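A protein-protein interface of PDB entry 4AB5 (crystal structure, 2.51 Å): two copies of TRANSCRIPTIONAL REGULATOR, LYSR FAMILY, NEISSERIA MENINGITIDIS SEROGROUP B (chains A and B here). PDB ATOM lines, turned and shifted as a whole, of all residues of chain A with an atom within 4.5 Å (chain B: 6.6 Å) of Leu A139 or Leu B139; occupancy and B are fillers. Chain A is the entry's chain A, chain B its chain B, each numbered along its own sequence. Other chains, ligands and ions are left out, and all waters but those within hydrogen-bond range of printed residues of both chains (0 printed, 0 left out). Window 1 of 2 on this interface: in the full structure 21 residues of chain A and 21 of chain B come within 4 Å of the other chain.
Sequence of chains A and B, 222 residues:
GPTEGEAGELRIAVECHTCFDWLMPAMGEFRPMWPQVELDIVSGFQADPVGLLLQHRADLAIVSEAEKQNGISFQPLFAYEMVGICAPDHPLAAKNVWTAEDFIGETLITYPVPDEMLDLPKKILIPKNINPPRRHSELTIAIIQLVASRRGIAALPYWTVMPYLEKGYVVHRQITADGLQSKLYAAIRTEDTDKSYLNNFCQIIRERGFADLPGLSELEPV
OG of Ser B137 is in hydrogen-bond range of O of Leu B139. The side-chain hydroxyl (OG) of Ser A137 lies within hydrogen-bond range of the backbone carbonyl oxygen (O) of Leu A139 (3.2 Å). The backbone carbonyl oxygen (O) of Glu B138 is in hydrogen-bond range of a ring nitrogen (ND1) of His B17 (3.4 Å).
Phe A20 touches Leu B139 (CG to CD1, 3.6 Å). CD1 of Ile B141 touches O of Phe A20, at 3.4 Å. CB of Ala B142 touches CE2 of Phe A20, 3.8 Å away. Glu B138 touches Glu A138. Glu A138 touches Leu B139 (O to CD2, 3.8 Å). CG of Phe B20 touches CD1 of Leu A139, at 3.7 Å. Glu B138 touches Leu A139. Leu B139 touches Leu A139. Ile A141 touches Phe B20 (CD1 to O, 3.4 Å). Phe B20 touches Ala A142 (CE2 to CB, 3.7 Å).
Leu A139 touches just these residues of chain B: Phe B20 (3.7 Å), Glu B138 (3.9 Å) and Leu B139 (3.8 Å). Leu B139 touches just these residues of chain A: Phe A20 (3.6 Å), Glu A138 (3.8 Å) and Leu A139 (3.8 Å). Of the printed residues of chain A, Glu B138 touches Glu A138 and Leu A139. Of the printed residues of chain A, Ile B141 touches Phe A20. Of the printed residues of chain A, Phe B20 touches Leu A139, Ile A141 and Ala A142. Of the printed residues of chain B, Phe A20 touches Leu B139, Ile B141 and Ala B142. Of the printed residues of chain B, Ala A142 touches Phe B20 (3.7 Å).
Of the 8 printed residues of chain A, 5 touch a printed residue of chain B. Printed residues of chain A that touch a printed residue of chain B: Phe A20, Glu A138, Leu A139, Ile A141 and Ala A142. Among the printed residues, 10 pairs touch across the chains.
Phe A20 touches Leu B139, and with the chains exchanged Leu A139 touches Phe B20. Phe A20 touches Ile B141, and with the chains exchanged Ile A141 touches Phe B20. Phe A20 touches Ala B142, and with the chains exchanged Ala A142 touches Phe B20. Glu A138 touches its own counterpart, Glu B138. Positions printed for both chains: 20, 137, 138, 139, 140, 141, 142 and 143. Of the 10 pairs that touch across the chains among the printed residues, 10 have their exchanged pair printed and touching as well.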
ATOM      1  N   PHE A  20     -28.616 -16.428 -13.689  1.00  0.00           N
ATOM      2  CA  PHE A  20     -28.242 -15.410 -12.704  1.00  0.00           C
ATOM      3  C   PHE A  20     -29.163 -14.186 -12.717  1.00  0.00           C
ATOM      4  O   PHE A  20     -29.400 -13.597 -11.663  1.00  0.00           O
ATOM      5  CB  PHE A  20     -26.765 -15.010 -12.874  1.00  0.00           C
ATOM      6  CG  PHE A  20     -25.782 -16.006 -12.298  1.00  0.00           C
ATOM      7  CD1 PHE A  20     -25.453 -17.167 -12.989  1.00  0.00           C
ATOM      8  CD2 PHE A  20     -25.163 -15.770 -11.075  1.00  0.00           C
ATOM      9  CE1 PHE A  20     -24.554 -18.090 -12.453  1.00  0.00           C
ATOM     10  CE2 PHE A  20     -24.257 -16.696 -10.541  1.00  0.00           C
ATOM     11  CZ  PHE A  20     -23.961 -17.850 -11.234  1.00  0.00           C
ATOM     12  N   SER A 137     -17.805 -14.660 -24.508  1.00  0.00           N
ATOM     13  CA  SER A 137     -17.977 -13.576 -23.553  1.00  0.00           C
ATOM     14  C   SER A 137     -18.724 -14.077 -22.326  1.00  0.00           C
ATOM     15  O   SER A 137     -19.707 -14.806 -22.457  1.00  0.00           O
ATOM     16  CB  SER A 137     -18.721 -12.397 -24.182  1.00  0.00           C
ATOM     17  OG  SER A 137     -18.810 -11.302 -23.283  1.00  0.00           O
ATOM     18  N   GLU A 138     -18.265 -13.665 -21.137  1.00  0.00           N
ATOM     19  CA  GLU A 138     -18.912 -13.995 -19.856  1.00  0.00           C
ATOM     20  C   GLU A 138     -20.153 -13.108 -19.636  1.00  0.00           C
ATOM     21  O   GLU A 138     -20.980 -13.427 -18.780  1.00  0.00           O
ATOM     22  CB  GLU A 138     -17.925 -13.787 -18.688  1.00  0.00           C
ATOM     23  CG  GLU A 138     -16.744 -14.753 -18.664  1.00  0.00           C
ATOM     24  CD  GLU A 138     -17.009 -16.169 -18.176  1.00  0.00           C
ATOM     25  OE1 GLU A 138     -18.041 -16.391 -17.504  1.00  0.00           O
ATOM     26  OE2 GLU A 138     -16.158 -17.051 -18.428  1.00  0.00           O
ATOM     27  N   LEU A 139     -20.269 -11.986 -20.392  1.00  0.00           N
ATOM     28  CA  LEU A 139     -21.339 -10.990 -20.240  1.00  0.00           C
ATOM     29  C   LEU A 139     -22.287 -10.902 -21.410  1.00  0.00           C
ATOM     30  O   LEU A 139     -21.846 -10.771 -22.546  1.00  0.00           O
ATOM     31  CB  LEU A 139     -20.758  -9.596 -19.917  1.00  0.00           C
ATOM     32  CG  LEU A 139     -19.646  -9.539 -18.849  1.00  0.00           C
ATOM     33  CD1 LEU A 139     -18.945  -8.189 -18.848  1.00  0.00           C
ATOM     34  CD2 LEU A 139     -20.175  -9.883 -17.465  1.00  0.00           C
ATOM     35  N   THR A 140     -23.597 -10.940 -21.118  1.00  0.00           N
ATOM     36  CA  THR A 140     -24.698 -10.860 -22.082  1.00  0.00           C
ATOM     37  C   THR A 140     -24.664  -9.518 -22.823  1.00  0.00           C
ATOM     38  O   THR A 140     -24.815  -9.485 -24.049  1.00  0.00           O
ATOM     39  CB  THR A 140     -26.034 -11.101 -21.356  1.00  0.00           C
ATOM     40  OG1 THR A 140     -26.023 -12.399 -20.763  1.00  0.00           O
ATOM     41  CG2 THR A 140     -27.231 -10.968 -22.264  1.00  0.00           C
ATOM     42  N   ILE A 141     -24.441  -8.422 -22.074  1.00  0.00           N
ATOM     43  CA  ILE A 141     -24.364  -7.060 -22.601  1.00  0.00           C
ATOM     44  C   ILE A 141     -23.274  -6.925 -23.673  1.00  0.00           C
ATOM     45  O   ILE A 141     -23.474  -6.196 -24.649  1.00  0.00           O
ATOM     46  CB  ILE A 141     -24.280  -5.990 -21.470  1.00  0.00           C
ATOM     47  CG1 ILE A 141     -22.991  -6.119 -20.618  1.00  0.00           C
ATOM     48  CG2 ILE A 141     -25.548  -5.997 -20.599  1.00  0.00           C
ATOM     49  CD1 ILE A 141     -22.745  -4.954 -19.658  1.00  0.00           C
ATOM     50  N   ALA A 142     -22.154  -7.674 -23.518  1.00  0.00           N
ATOM     51  CA  ALA A 142     -21.048  -7.697 -24.472  1.00  0.00           C
ATOM     52  C   ALA A 142     -21.420  -8.546 -25.687  1.00  0.00           C
ATOM     53  O   ALA A 142     -21.087  -8.158 -26.805  1.00  0.00           O
ATOM     54  CB  ALA A 142     -19.781  -8.211 -23.811  1.00  0.00           C
ATOM     55  N   ILE A 143     -22.149  -9.672 -25.476  1.00  0.00           N
ATOM     56  CA  ILE A 143     -22.637 -10.533 -26.567  1.00  0.00           C
ATOM     57  C   ILE A 143     -23.519  -9.710 -27.524  1.00  0.00           C
ATOM     58  O   ILE A 143     -23.259  -9.716 -28.723  1.00  0.00           O
ATOM     59  CB  ILE A 143     -23.353 -11.833 -26.068  1.00  0.00           C
ATOM     60  CG1 ILE A 143     -22.336 -12.786 -25.373  1.00  0.00           C
ATOM     61  CG2 ILE A 143     -24.098 -12.548 -27.230  1.00  0.00           C
ATOM     62  CD1 ILE A 143     -22.932 -14.035 -24.706  1.00  0.00           C
ATOM     63  N   CYS B  16     -11.491  -4.434 -17.793  1.00  0.00           N
ATOM     64  CA  CYS B  16     -12.224  -4.021 -16.596  1.00  0.00           C
ATOM     65  C   CYS B  16     -13.704  -4.417 -16.704  1.00  0.00           C
ATOM     66  O   CYS B  16     -14.372  -4.047 -17.673  1.00  0.00           O
ATOM     67  CB  CYS B  16     -12.022  -2.520 -16.363  1.00  0.00           C
ATOM     68  SG  CYS B  16     -13.425  -1.638 -15.604  1.00  0.00           S
ATOM     69  N   HIS B  17     -14.198  -5.190 -15.715  1.00  0.00           N
ATOM     70  CA  HIS B  17     -15.564  -5.729 -15.656  1.00  0.00           C
ATOM     71  C   HIS B  17     -16.676  -4.685 -15.490  1.00  0.00           C
ATOM     72  O   HIS B  17     -17.638  -4.715 -16.259  1.00  0.00           O
ATOM     73  CB  HIS B  17     -15.654  -6.803 -14.565  1.00  0.00           C
ATOM     74  CG  HIS B  17     -14.905  -8.067 -14.866  1.00  0.00           C
ATOM     75  ND1 HIS B  17     -15.565  -9.276 -15.017  1.00  0.00           N
ATOM     76  CD2 HIS B  17     -13.572  -8.284 -14.973  1.00  0.00           C
ATOM     77  CE1 HIS B  17     -14.623 -10.178 -15.233  1.00  0.00           C
ATOM     78  NE2 HIS B  17     -13.408  -9.632 -15.214  1.00  0.00           N
ATOM     79  N   PHE B  20     -18.012  -2.266 -18.574  1.00  0.00           N
ATOM     80  CA  PHE B  20     -19.048  -2.759 -19.487  1.00  0.00           C
ATOM     81  C   PHE B  20     -20.438  -2.166 -19.229  1.00  0.00           C
ATOM     82  O   PHE B  20     -21.203  -1.969 -20.182  1.00  0.00           O
ATOM     83  CB  PHE B  20     -19.084  -4.295 -19.471  1.00  0.00           C
ATOM     84  CG  PHE B  20     -17.985  -4.958 -20.267  1.00  0.00           C
ATOM     85  CD1 PHE B  20     -16.704  -5.097 -19.736  1.00  0.00           C
ATOM     86  CD2 PHE B  20     -18.231  -5.454 -21.544  1.00  0.00           C
ATOM     87  CE1 PHE B  20     -15.682  -5.712 -20.479  1.00  0.00           C
ATOM     88  CE2 PHE B  20     -17.208  -6.050 -22.293  1.00  0.00           C
ATOM     89  CZ  PHE B  20     -15.943  -6.184 -21.752  1.00  0.00           C
ATOM     90  N   TYR B 111     -13.329  -9.997  -9.119  1.00  0.00           N
ATOM     91  CA  TYR B 111     -13.449 -10.540 -10.472  1.00  0.00           C
ATOM     92  C   TYR B 111     -12.269 -11.508 -10.674  1.00  0.00           C
ATOM     93  O   TYR B 111     -11.248 -11.342  -9.995  1.00  0.00           O
ATOM     94  CB  TYR B 111     -13.471  -9.423 -11.527  1.00  0.00           C
ATOM     95  CG  TYR B 111     -14.647  -8.493 -11.348  1.00  0.00           C
ATOM     96  CD1 TYR B 111     -15.944  -8.915 -11.631  1.00  0.00           C
ATOM     97  CD2 TYR B 111     -14.477  -7.211 -10.835  1.00  0.00           C
ATOM     98  CE1 TYR B 111     -17.039  -8.069 -11.443  1.00  0.00           C
ATOM     99  CE2 TYR B 111     -15.566  -6.357 -10.636  1.00  0.00           C
ATOM    100  CZ  TYR B 111     -16.845  -6.792 -10.943  1.00  0.00           C
ATOM    101  OH  TYR B 111     -17.922  -5.960 -10.751  1.00  0.00           O
ATOM    102  N   PRO B 112     -12.393 -12.568 -11.520  1.00  0.00           N
ATOM    103  CA  PRO B 112     -11.295 -13.551 -11.644  1.00  0.00           C
ATOM    104  C   PRO B 112     -10.184 -13.017 -12.534  1.00  0.00           C
ATOM    105  O   PRO B 112     -10.052 -13.372 -13.714  1.00  0.00           O
ATOM    106  CB  PRO B 112     -11.994 -14.799 -12.220  1.00  0.00           C
ATOM    107  CG  PRO B 112     -13.465 -14.459 -12.253  1.00  0.00           C
ATOM    108  CD  PRO B 112     -13.531 -12.972 -12.361  1.00  0.00           C
ATOM    109  N   SER B 137     -15.812 -14.218  -8.978  1.00  0.00           N
ATOM    110  CA  SER B 137     -17.017 -14.219  -9.801  1.00  0.00           C
ATOM    111  C   SER B 137     -16.852 -13.252 -10.970  1.00  0.00           C
ATOM    112  O   SER B 137     -16.351 -12.143 -10.794  1.00  0.00           O
ATOM    113  CB  SER B 137     -18.249 -13.847  -8.976  1.00  0.00           C
ATOM    114  OG  SER B 137     -19.427 -13.956  -9.756  1.00  0.00           O
ATOM    115  N   GLU B 138     -17.289 -13.677 -12.160  1.00  0.00           N
ATOM    116  CA  GLU B 138     -17.280 -12.858 -13.377  1.00  0.00           C
ATOM    117  C   GLU B 138     -18.453 -11.861 -13.361  1.00  0.00           C
ATOM    118  O   GLU B 138     -18.441 -10.909 -14.134  1.00  0.00           O
ATOM    119  CB  GLU B 138     -17.396 -13.757 -14.627  1.00  0.00           C
ATOM    120  CG  GLU B 138     -16.196 -14.664 -14.877  1.00  0.00           C
ATOM    121  CD  GLU B 138     -14.954 -14.019 -15.475  1.00  0.00           C
ATOM    122  OE1 GLU B 138     -15.046 -12.894 -16.016  1.00  0.00           O
ATOM    123  OE2 GLU B 138     -13.886 -14.671 -15.437  1.00  0.00           O
ATOM    124  N   LEU B 139     -19.472 -12.090 -12.496  1.00  0.00           N
ATOM    125  CA  LEU B 139     -20.696 -11.290 -12.423  1.00  0.00           C
ATOM    126  C   LEU B 139     -20.856 -10.505 -11.140  1.00  0.00           C
ATOM    127  O   LEU B 139     -20.748 -11.071 -10.053  1.00  0.00           O
ATOM    128  CB  LEU B 139     -21.942 -12.176 -12.667  1.00  0.00           C
ATOM    129  CG  LEU B 139     -21.877 -13.171 -13.838  1.00  0.00           C
ATOM    130  CD1 LEU B 139     -23.012 -14.164 -13.784  1.00  0.00           C
ATOM    131  CD2 LEU B 139     -21.831 -12.463 -15.183  1.00  0.00           C
ATOM    132  N   THR B 140     -21.162  -9.202 -11.274  1.00  0.00           N
ATOM    133  CA  THR B 140     -21.381  -8.251 -10.179  1.00  0.00           C
ATOM    134  C   THR B 140     -22.565  -8.682  -9.320  1.00  0.00           C
ATOM    135  O   THR B 140     -22.474  -8.667  -8.095  1.00  0.00           O
ATOM    136  CB  THR B 140     -21.555  -6.833 -10.759  1.00  0.00           C
ATOM    137  OG1 THR B 140     -20.371  -6.464 -11.467  1.00  0.00           O
ATOM    138  CG2 THR B 140     -21.866  -5.793  -9.701  1.00  0.00           C
ATOM    139  N   ILE B 141     -23.666  -9.085  -9.974  1.00  0.00           N
ATOM    140  CA  ILE B 141     -24.895  -9.549  -9.328  1.00  0.00           C
ATOM    141  C   ILE B 141     -24.635 -10.744  -8.388  1.00  0.00           C
ATOM    142  O   ILE B 141     -25.252 -10.825  -7.325  1.00  0.00           O
ATOM    143  CB  ILE B 141     -26.055  -9.780 -10.336  1.00  0.00           C
ATOM    144  CG1 ILE B 141     -25.722 -10.879 -11.384  1.00  0.00           C
ATOM    145  CG2 ILE B 141     -26.465  -8.457 -11.001  1.00  0.00           C
ATOM    146  CD1 ILE B 141     -26.902 -11.336 -12.250  1.00  0.00           C
ATOM    147  N   ALA B 142     -23.682 -11.623  -8.762  1.00  0.00           N
ATOM    148  CA  ALA B 142     -23.283 -12.774  -7.958  1.00  0.00           C
ATOM    149  C   ALA B 142     -22.391 -12.327  -6.793  1.00  0.00           C
ATOM    150  O   ALA B 142     -22.553 -12.851  -5.696  1.00  0.00           O
ATOM    151  CB  ALA B 142     -22.577 -13.809  -8.817  1.00  0.00           C
ATOM    152  N   ILE B 143     -21.488 -11.331  -7.018  1.00  0.00           N
ATOM    153  CA  ILE B 143     -20.643 -10.754  -5.967  1.00  0.00           C
ATOM    154  C   ILE B 143     -21.517 -10.199  -4.833  1.00  0.00           C
ATOM    155  O   ILE B 143     -21.306 -10.574  -3.680  1.00  0.00           O
ATOM    156  CB  ILE B 143     -19.623  -9.700  -6.498  1.00  0.00           C
ATOM    157  CG1 ILE B 143     -18.555 -10.373  -7.413  1.00  0.00           C
ATOM    158  CG2 ILE B 143     -18.952  -8.928  -5.322  1.00  0.00           C
ATOM    159  CD1 ILE B 143     -17.567  -9.434  -8.114  1.00  0.00           C
ATOM    160  N   ILE B 144     -22.521  -9.350  -5.173  1.00  0.00           N
ATOM    161  CA  ILE B 144     -23.450  -8.740  -4.226  1.00  0.00           C
ATOM    162  C   ILE B 144     -24.221  -9.772  -3.417  1.00  0.00           C
ATOM    163  O   ILE B 144     -24.295  -9.631  -2.195  1.00  0.00           O
ATOM    164  CB  ILE B 144     -24.323  -7.622  -4.893  1.00  0.00           C
ATOM    165  CG1 ILE B 144     -23.554  -6.290  -4.901  1.00  0.00           C
ATOM    166  CG2 ILE B 144     -25.699  -7.430  -4.211  1.00  0.00           C
ATOM    167  CD1 ILE B 144     -23.148  -5.862  -6.186  1.00  0.00           C
